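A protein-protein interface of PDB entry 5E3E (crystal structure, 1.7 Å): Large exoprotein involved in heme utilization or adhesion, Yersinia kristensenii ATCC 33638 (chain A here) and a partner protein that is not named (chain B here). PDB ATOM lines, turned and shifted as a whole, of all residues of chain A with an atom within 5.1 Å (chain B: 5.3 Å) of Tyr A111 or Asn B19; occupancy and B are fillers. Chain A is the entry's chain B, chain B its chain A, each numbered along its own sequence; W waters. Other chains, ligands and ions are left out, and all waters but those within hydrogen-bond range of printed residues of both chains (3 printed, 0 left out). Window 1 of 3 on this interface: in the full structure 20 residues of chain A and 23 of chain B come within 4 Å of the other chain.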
ATOM      1  N   HIS A   8       8.189  -5.855 -27.628  1.00  0.00           N
ATOM      2  CA  HIS A   8       7.725  -6.609 -26.430  1.00  0.00           C
ATOM      3  C   HIS A   8       8.703  -7.709 -26.059  1.00  0.00           C
ATOM      4  O   HIS A   8       8.310  -8.754 -25.505  1.00  0.00           O
ATOM      5  CB  HIS A   8       6.339  -7.191 -26.670  1.00  0.00           C
ATOM      6  CG  HIS A   8       5.368  -6.170 -27.150  1.00  0.00           C
ATOM      7  ND1 HIS A   8       4.742  -5.292 -26.307  1.00  0.00           N
ATOM      8  CD2 HIS A   8       4.969  -5.836 -28.403  1.00  0.00           C
ATOM      9  CE1 HIS A   8       3.973  -4.478 -27.010  1.00  0.00           C
ATOM     10  NE2 HIS A   8       4.120  -4.768 -28.287  1.00  0.00           N
ATOM     11  N   SER A  29       3.393  -4.624 -21.857  1.00  0.00           N
ATOM     12  CA  SER A  29       4.090  -5.810 -21.398  1.00  0.00           C
ATOM     13  C   SER A  29       5.228  -6.220 -22.340  1.00  0.00           C
ATOM     14  O   SER A  29       5.300  -5.781 -23.501  1.00  0.00           O
ATOM     15  CB  SER A  29       3.079  -6.935 -21.255  1.00  0.00           C
ATOM     16  OG  SER A  29       2.527  -7.283 -22.534  1.00  0.00           O
ATOM     17  N   PHE A  31       8.050  -9.803 -23.007  1.00  0.00           N
ATOM     18  CA  PHE A  31       8.677 -11.088 -22.699  1.00  0.00           C
ATOM     19  C   PHE A  31      10.044 -10.830 -22.073  1.00  0.00           C
ATOM     20  O   PHE A  31      10.704  -9.833 -22.360  1.00  0.00           O
ATOM     21  CB  PHE A  31       8.877 -11.935 -23.948  1.00  0.00           C
ATOM     22  CG  PHE A  31       7.601 -12.369 -24.592  1.00  0.00           C
ATOM     23  CD1 PHE A  31       6.803 -13.352 -23.995  1.00  0.00           C
ATOM     24  CD2 PHE A  31       7.172 -11.780 -25.769  1.00  0.00           C
ATOM     25  CE1 PHE A  31       5.641 -13.758 -24.592  1.00  0.00           C
ATOM     26  CE2 PHE A  31       6.023 -12.189 -26.365  1.00  0.00           C
ATOM     27  CZ  PHE A  31       5.236 -13.172 -25.762  1.00  0.00           C
ATOM     28  N   ASN A  90       0.752 -15.749 -18.977  1.00  0.00           N
ATOM     29  CA  ASN A  90       0.011 -16.003 -20.211  1.00  0.00           C
ATOM     30  C   ASN A  90       0.494 -15.082 -21.334  1.00  0.00           C
ATOM     31  O   ASN A  90       1.180 -14.121 -21.082  1.00  0.00           O
ATOM     32  CB  ASN A  90      -1.447 -15.729 -19.979  1.00  0.00           C
ATOM     33  CG  ASN A  90      -2.072 -16.714 -19.026  1.00  0.00           C
ATOM     34  OD1 ASN A  90      -1.483 -17.736 -18.677  1.00  0.00           O
ATOM     35  ND2 ASN A  90      -3.313 -16.415 -18.618  1.00  0.00           N
ATOM     36  N   ALA A  91       0.092 -15.361 -22.560  1.00  0.00           N
ATOM     37  CA  ALA A  91       0.483 -14.514 -23.687  1.00  0.00           C
ATOM     38  C   ALA A  91      -0.513 -14.510 -24.817  1.00  0.00           C
ATOM     39  O   ALA A  91      -1.366 -15.375 -24.898  1.00  0.00           O
ATOM     40  CB  ALA A  91       1.832 -14.948 -24.220  1.00  0.00           C
ATOM     41  N   ARG A  92      -0.348 -13.582 -25.741  1.00  0.00           N
ATOM     42  CA  ARG A  92      -1.251 -13.505 -26.882  1.00  0.00           C
ATOM     43  C   ARG A  92      -0.359 -13.229 -28.048  1.00  0.00           C
ATOM     44  O   ARG A  92       0.512 -12.367 -27.989  1.00  0.00           O
ATOM     45  CB  ARG A  92      -2.271 -12.386 -26.704  1.00  0.00           C
ATOM     46  CG  ARG A  92      -3.237 -12.197 -27.879  1.00  0.00           C
ATOM     47  CD  ARG A  92      -4.285 -11.108 -27.617  1.00  0.00           C
ATOM     48  NE  ARG A  92      -5.076 -11.531 -26.456  1.00  0.00           N
ATOM     49  CZ  ARG A  92      -5.405 -10.765 -25.422  1.00  0.00           C
ATOM     50  NH1 ARG A  92      -5.095  -9.477 -25.379  1.00  0.00           N
ATOM     51  NH2 ARG A  92      -6.097 -11.301 -24.431  1.00  0.00           N
ATOM     52  N   ILE A  93      -0.610 -13.956 -29.129  1.00  0.00           N
ATOM     53  CA  ILE A  93       0.055 -13.725 -30.395  1.00  0.00           C
ATOM     54  C   ILE A  93      -0.991 -13.328 -31.412  1.00  0.00           C
ATOM     55  O   ILE A  93      -2.078 -13.885 -31.408  1.00  0.00           O
ATOM     56  CB  ILE A  93       0.747 -15.035 -30.904  1.00  0.00           C
ATOM     57  CG1 ILE A  93       1.635 -15.688 -29.815  1.00  0.00           C
ATOM     58  CG2 ILE A  93       1.506 -14.774 -32.186  1.00  0.00           C
ATOM     59  CD1 ILE A  93       2.656 -14.850 -29.188  1.00  0.00           C
ATOM     60  N   ILE A  94      -0.685 -12.375 -32.283  1.00  0.00           N
ATOM     61  CA  ILE A  94      -1.615 -12.010 -33.349  1.00  0.00           C
ATOM     62  C   ILE A  94      -0.956 -12.356 -34.660  1.00  0.00           C
ATOM     63  O   ILE A  94       0.170 -11.893 -34.917  1.00  0.00           O
ATOM     64  CB  ILE A  94      -1.955 -10.498 -33.355  1.00  0.00           C
ATOM     65  CG1 ILE A  94      -2.567 -10.030 -32.024  1.00  0.00           C
ATOM     66  CG2 ILE A  94      -2.896 -10.141 -34.520  1.00  0.00           C
ATOM     67  CD1 ILE A  94      -3.730 -10.841 -31.565  1.00  0.00           C
ATOM     68  N   THR A 109       2.299  -9.456 -34.120  1.00  0.00           N
ATOM     69  CA  THR A 109       2.908  -9.089 -32.829  1.00  0.00           C
ATOM     70  C   THR A 109       2.550 -10.132 -31.789  1.00  0.00           C
ATOM     71  O   THR A 109       1.850 -11.101 -32.075  1.00  0.00           O
ATOM     72  CB  THR A 109       2.451  -7.677 -32.372  1.00  0.00           C
ATOM     73  OG1 THR A 109       3.261  -7.202 -31.277  1.00  0.00           O
ATOM     74  CG2 THR A 109       1.012  -7.646 -32.029  1.00  0.00           C
ATOM     75  N   GLY A 110       3.084  -9.942 -30.596  1.00  0.00           N
ATOM     76  CA  GLY A 110       2.721 -10.810 -29.484  1.00  0.00           C
ATOM     77  C   GLY A 110       3.335 -10.269 -28.205  1.00  0.00           C
ATOM     78  O   GLY A 110       4.311  -9.548 -28.246  1.00  0.00           O
ATOM     79  N   TYR A 111       2.746 -10.644 -27.066  1.00  0.00           N
ATOM     80  CA  TYR A 111       3.202 -10.141 -25.782  1.00  0.00           C
ATOM     81  C   TYR A 111       2.528 -10.857 -24.633  1.00  0.00           C
ATOM     82  O   TYR A 111       1.477 -11.488 -24.807  1.00  0.00           O
ATOM     83  CB  TYR A 111       2.934  -8.645 -25.644  1.00  0.00           C
ATOM     84  CG  TYR A 111       1.601  -8.138 -26.208  1.00  0.00           C
ATOM     85  CD1 TYR A 111       0.385  -8.384 -25.561  1.00  0.00           C
ATOM     86  CD2 TYR A 111       1.591  -7.414 -27.384  1.00  0.00           C
ATOM     87  CE1 TYR A 111      -0.818  -7.902 -26.106  1.00  0.00           C
ATOM     88  CE2 TYR A 111       0.426  -6.909 -27.917  1.00  0.00           C
ATOM     89  CZ  TYR A 111      -0.768  -7.159 -27.268  1.00  0.00           C
ATOM     90  OH  TYR A 111      -1.877  -6.623 -27.841  1.00  0.00           O
ATOM     91  N   PRO A 112       3.096 -10.719 -23.431  1.00  0.00           N
ATOM     92  CA  PRO A 112       2.444 -11.357 -22.279  1.00  0.00           C
ATOM     93  C   PRO A 112       1.110 -10.694 -21.954  1.00  0.00           C
ATOM     94  O   PRO A 112       0.938  -9.493 -22.235  1.00  0.00           O
ATOM     95  CB  PRO A 112       3.426 -11.133 -21.143  1.00  0.00           C
ATOM     96  CG  PRO A 112       4.753 -10.884 -21.793  1.00  0.00           C
ATOM     97  CD  PRO A 112       4.446 -10.234 -23.112  1.00  0.00           C
ATOM     98  N   THR A 113       0.201 -11.464 -21.360  1.00  0.00           N
ATOM     99  CA  THR A 113      -1.094 -10.955 -20.947  1.00  0.00           C
ATOM    100  C   THR A 113      -1.344 -11.384 -19.514  1.00  0.00           C
ATOM    101  O   THR A 113      -1.069 -12.507 -19.170  1.00  0.00           O
ATOM    102  CB  THR A 113      -2.241 -11.449 -21.862  1.00  0.00           C
ATOM    103  OG1 THR A 113      -2.211 -12.881 -21.989  1.00  0.00           O
ATOM    104  CG2 THR A 113      -2.128 -10.850 -23.246  1.00  0.00           C
ATOM    105  N   LEU B  14     -11.152  -5.513 -30.172  1.00  0.00           N
ATOM    106  CA  LEU B  14     -10.454  -4.932 -29.052  1.00  0.00           C
ATOM    107  C   LEU B  14      -9.103  -5.597 -28.792  1.00  0.00           C
ATOM    108  O   LEU B  14      -8.198  -4.937 -28.282  1.00  0.00           O
ATOM    109  CB  LEU B  14     -11.335  -4.947 -27.793  1.00  0.00           C
ATOM    110  CG  LEU B  14     -12.586  -4.061 -27.871  1.00  0.00           C
ATOM    111  CD1 LEU B  14     -13.407  -4.069 -26.589  1.00  0.00           C
ATOM    112  CD2 LEU B  14     -12.285  -2.646 -28.305  1.00  0.00           C
ATOM    113  N   ARG B  15      -8.956  -6.845 -29.212  1.00  0.00           N
ATOM    114  CA  ARG B  15      -7.716  -7.569 -29.011  1.00  0.00           C
ATOM    115  C   ARG B  15      -6.818  -7.614 -30.218  1.00  0.00           C
ATOM    116  O   ARG B  15      -5.599  -7.612 -30.043  1.00  0.00           O
ATOM    117  CB  ARG B  15      -7.953  -8.968 -28.503  1.00  0.00           C
ATOM    118  CG  ARG B  15      -8.686  -8.997 -27.200  1.00  0.00           C
ATOM    119  CD  ARG B  15      -8.903 -10.420 -26.747  1.00  0.00           C
ATOM    120  NE  ARG B  15      -9.659 -10.518 -25.492  1.00  0.00           N
ATOM    121  CZ  ARG B  15      -9.889 -11.666 -24.841  1.00  0.00           C
ATOM    122  NH1 ARG B  15      -9.439 -12.839 -25.302  1.00  0.00           N
ATOM    123  NH2 ARG B  15     -10.611 -11.660 -23.735  1.00  0.00           N
ATOM    124  N   CYS B  16      -7.367  -7.670 -31.425  1.00  0.00           N
ATOM    125  CA  CYS B  16      -6.536  -7.786 -32.607  1.00  0.00           C
ATOM    126  C   CYS B  16      -6.253  -6.414 -33.205  1.00  0.00           C
ATOM    127  O   CYS B  16      -5.180  -6.223 -33.801  1.00  0.00           O
ATOM    128  CB  CYS B  16      -7.138  -8.709 -33.656  1.00  0.00           C
ATOM    129  SG  CYS B  16      -7.087 -10.452 -33.184  1.00  0.00           S
ATOM    130  N   TYR B  17      -7.237  -5.505 -33.172  1.00  0.00           N
ATOM    131  CA  TYR B  17      -7.035  -4.185 -33.718  1.00  0.00           C
ATOM    132  C   TYR B  17      -6.514  -3.264 -32.635  1.00  0.00           C
ATOM    133  O   TYR B  17      -5.465  -2.655 -32.844  1.00  0.00           O
ATOM    134  CB  TYR B  17      -8.305  -3.623 -34.394  1.00  0.00           C
ATOM    135  CG  TYR B  17      -8.467  -4.196 -35.788  1.00  0.00           C
ATOM    136  CD1 TYR B  17      -9.029  -5.444 -35.995  1.00  0.00           C
ATOM    137  CD2 TYR B  17      -7.983  -3.477 -36.908  1.00  0.00           C
ATOM    138  CE1 TYR B  17      -9.116  -5.974 -37.268  1.00  0.00           C
ATOM    139  CE2 TYR B  17      -8.103  -3.976 -38.176  1.00  0.00           C
ATOM    140  CZ  TYR B  17      -8.667  -5.222 -38.359  1.00  0.00           C
ATOM    141  OH  TYR B  17      -8.756  -5.730 -39.635  1.00  0.00           O
ATOM    142  N   PHE B  18      -7.225  -3.146 -31.515  1.00  0.00           N
ATOM    143  CA  PHE B  18      -6.710  -2.338 -30.398  1.00  0.00           C
ATOM    144  C   PHE B  18      -5.688  -3.072 -29.560  1.00  0.00           C
ATOM    145  O   PHE B  18      -5.720  -3.038 -28.340  1.00  0.00           O
ATOM    146  CB  PHE B  18      -7.824  -1.710 -29.574  1.00  0.00           C
ATOM    147  CG  PHE B  18      -8.578  -0.645 -30.310  1.00  0.00           C
ATOM    148  CD1 PHE B  18      -8.027   0.599 -30.491  1.00  0.00           C
ATOM    149  CD2 PHE B  18      -9.814  -0.909 -30.877  1.00  0.00           C
ATOM    150  CE1 PHE B  18      -8.718   1.588 -31.176  1.00  0.00           C
ATOM    151  CE2 PHE B  18     -10.520   0.091 -31.567  1.00  0.00           C
ATOM    152  CZ  PHE B  18      -9.949   1.330 -31.717  1.00  0.00           C
ATOM    153  N   ASN B  19      -4.749  -3.738 -30.243  1.00  0.00           N
ATOM    154  CA  ASN B  19      -3.612  -4.362 -29.594  1.00  0.00           C
ATOM    155  C   ASN B  19      -2.630  -3.278 -29.093  1.00  0.00           C
ATOM    156  O   ASN B  19      -2.786  -2.109 -29.385  1.00  0.00           O
ATOM    157  CB  ASN B  19      -2.941  -5.398 -30.506  1.00  0.00           C
ATOM    158  CG  ASN B  19      -2.260  -4.776 -31.692  1.00  0.00           C
ATOM    159  OD1 ASN B  19      -1.299  -4.036 -31.541  1.00  0.00           O
ATOM    160  ND2 ASN B  19      -2.756  -5.064 -32.897  1.00  0.00           N
ATOM    161  N   GLN B  20      -1.632  -3.665 -28.291  1.00  0.00           N
ATOM    162  CA  GLN B  20      -0.720  -2.676 -27.720  1.00  0.00           C
ATOM    163  C   GLN B  20       0.039  -1.862 -28.767  1.00  0.00           C
ATOM    164  O   GLN B  20       0.545  -0.772 -28.466  1.00  0.00           O
ATOM    165  CB  GLN B  20       0.309  -3.354 -26.806  1.00  0.00           C
ATOM    166  CG  GLN B  20      -0.290  -3.839 -25.509  1.00  0.00           C
ATOM    167  CD  GLN B  20       0.740  -4.458 -24.573  1.00  0.00           C
ATOM    168  OE1 GLN B  20       1.910  -4.055 -24.535  1.00  0.00           O
ATOM    169  NE2 GLN B  20       0.302  -5.431 -23.794  1.00  0.00           N
ATOM    170  N   ASP B  21       0.138  -2.403 -29.972  1.00  0.00           N
ATOM    171  CA  ASP B  21       0.843  -1.746 -31.056  1.00  0.00           C
ATOM    172  C   ASP B  21      -0.056  -1.021 -32.067  1.00  0.00           C
ATOM    173  O   ASP B  21       0.403  -0.696 -33.168  1.00  0.00           O
ATOM    174  CB  ASP B  21       1.682  -2.771 -31.791  1.00  0.00           C
ATOM    175  CG  ASP B  21       2.558  -3.582 -30.853  1.00  0.00           C
ATOM    176  OD1 ASP B  21       3.221  -2.990 -30.002  1.00  0.00           O
ATOM    177  OD2 ASP B  21       2.551  -4.805 -30.956  1.00  0.00           O
ATOM    178  N   PHE B  22      -1.279  -0.684 -31.691  1.00  0.00           N
ATOM    179  CA  PHE B  22      -2.228  -0.067 -32.652  1.00  0.00           C
ATOM    180  C   PHE B  22      -1.733   1.242 -33.274  1.00  0.00           C
ATOM    181  O   PHE B  22      -2.013   1.503 -34.426  1.00  0.00           O
ATOM    182  CB  PHE B  22      -3.623   0.098 -32.048  1.00  0.00           C
ATOM    183  CG  PHE B  22      -3.775   1.273 -31.113  1.00  0.00           C
ATOM    184  CD1 PHE B  22      -3.475   1.144 -29.773  1.00  0.00           C
ATOM    185  CD2 PHE B  22      -4.276   2.501 -31.573  1.00  0.00           C
ATOM    186  CE1 PHE B  22      -3.637   2.214 -28.889  1.00  0.00           C
ATOM    187  CE2 PHE B  22      -4.434   3.568 -30.696  1.00  0.00           C
ATOM    188  CZ  PHE B  22      -4.080   3.427 -29.358  1.00  0.00           C
ATOM    189  N   LEU B  25       0.820   0.080 -36.041  1.00  0.00           N
ATOM    190  CA  LEU B  25       0.174  -0.675 -37.101  1.00  0.00           C
ATOM    191  C   LEU B  25      -0.818   0.130 -37.884  1.00  0.00           C
ATOM    192  O   LEU B  25      -0.861   0.030 -39.107  1.00  0.00           O
ATOM    193  CB  LEU B  25      -0.600  -1.880 -36.556  1.00  0.00           C
ATOM    194  CG  LEU B  25       0.224  -3.078 -36.192  1.00  0.00           C
ATOM    195  CD1 LEU B  25      -0.622  -3.998 -35.294  1.00  0.00           C
ATOM    196  CD2 LEU B  25       0.701  -3.787 -37.459  1.00  0.00           C
ATOM    197  N   PHE B  26      -1.653   0.902 -37.188  1.00  0.00           N
ATOM    198  CA  PHE B  26      -2.785   1.545 -37.849  1.00  0.00           C
ATOM    199  C   PHE B  26      -2.817   3.061 -37.721  1.00  0.00           C
ATOM    200  O   PHE B  26      -3.246   3.769 -38.639  1.00  0.00           O
ATOM    201  CB  PHE B  26      -4.094   0.979 -37.281  1.00  0.00           C
ATOM    202  CG  PHE B  26      -4.180  -0.523 -37.301  1.00  0.00           C
ATOM    203  CD1 PHE B  26      -4.184  -1.218 -38.504  1.00  0.00           C
ATOM    204  CD2 PHE B  26      -4.269  -1.241 -36.122  1.00  0.00           C
ATOM    205  CE1 PHE B  26      -4.330  -2.603 -38.531  1.00  0.00           C
ATOM    206  CE2 PHE B  26      -4.389  -2.612 -36.130  1.00  0.00           C
ATOM    207  CZ  PHE B  26      -4.422  -3.308 -37.333  1.00  0.00           C
ATOM    208  N   SER B  76      -6.519  -2.614 -25.438  1.00  0.00           N
ATOM    209  CA  SER B  76      -5.225  -1.967 -25.014  1.00  0.00           C
ATOM    210  C   SER B  76      -5.283  -0.443 -25.073  1.00  0.00           C
ATOM    211  O   SER B  76      -4.495   0.229 -24.408  1.00  0.00           O
ATOM    212  CB  SER B  76      -4.052  -2.418 -25.902  1.00  0.00           C
ATOM    213  OG  SER B  76      -3.846  -3.810 -25.782  1.00  0.00           O
HETATM  214  O   HOH W   1      -4.386  -7.687 -27.584  1.00  0.00           O
HETATM  215  O   HOH W   2      -0.947  -7.478 -22.040  1.00  0.00           O
HETATM  216  O   HOH W   3      -6.503 -13.920 -23.776  1.00  0.00           O
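CE1 of His A8 touches OE1 of Gln B20 (3.2 Å).
Arg A92 touches Arg B15.
Cys B16 touches Ile A94 (SG to CD1, 3.7 Å).
Tyr A111 touches Asn B19 (OH to CB, 3.1 Å).
The side-chain carboxylate (OD2) of Asp B21 is in hydrogen-bond range of the side-chain hydroxyl (OG1) of Thr A109 (2.5 Å).
OH of Tyr A111 lies within hydrogen-bond range of N of Gln B20 (3.0 Å).
NE2 of His A8 sits at hydrogen-bond distance from OD1 of Asp B21 (2.6 Å).
The side-chain amide oxygen (OE1) of Gln B20 is in hydrogen-bond range of the backbone NH (N) of Ser A29, 3.1 Å away.
The side-chain amide oxygen of Asn B19 lies within hydrogen-bond range of the backbone NH of Phe B22, at 3.4 Å.
The backbone carbonyl oxygen of Pro A112 is in hydrogen-bond range of the side-chain hydroxyl of Ser A29 (2.7 Å).
OD1 of Asn B19 is in hydrogen-bond range of N of Asp B21 (2.7 Å).
N of Phe A31 lies within hydrogen-bond range of O of His A8 (2.7 Å).
A ring nitrogen (ND1) of His A8 sits at hydrogen-bond distance from the backbone carbonyl oxygen (O) of Ser A29 (2.9 Å).
O of Cys B16 lies within hydrogen-bond range of ND2 of Asn B19 (2.8 Å).
Water W3 lies within hydrogen-bond range of the guanidinium group (NH2) of Arg A92 (2.7 Å) and the guanidinium group (NH1) of Arg B15 (3.5 Å).
Water W1 lies within hydrogen-bond range of OH of Tyr A111 (2.7 Å), O of Arg B15 (2.7 Å) and NH1 of Arg A92 (2.9 Å).
Water W2 bridges the backbone carbonyl oxygen (O) of Pro A112 and the side-chain amide nitrogen (NE2) of Gln B20.
Printed residues of chain B that touch a printed residue of chain A: Arg B15, Cys B16, Asn B19, Gln B20 and Asp B21.
Hydrophobic or aromatic side chains of chain A within 4 Å of the printed part of chain B: His A8, Ile A94 and Tyr A111.
Among the printed residues, 8 pairs touch across the chains.
Among the printed residues, no Asp or Glu carboxylate lies within 4 Å of a Lys or Arg side-chain nitrogen of the other chain.
Printed residues of chain B within 4 Å of Tyr A111: Asn B19 (3.1 Å) and Gln B20 (3.0 Å).
Of chain A, only Tyr A111 (3.1 Å) comes within 4 Å of Asn B19.
Of the printed residues of chain A, Gln B20 touches His A8, Ser A29 and Tyr A111.
Printed residues of chain A within 4 Å of Cys B16: Ile A94.
Of the printed residues of chain B, Ser A29 touches Gln B20.
Printed residues of chain B within 4 Å of Thr A109: Asp B21.
Of the printed residues of chain B, His A8 touches Gln B20 (3.2 Å) and Asp B21 (2.6 Å).
The nearest residue of chain A that does not touch Asn B19 is Thr A109 (4.3 Å).
The nearest printed residue of chain A that does not touch Arg B15 is Ile A94 (4.03 Å).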
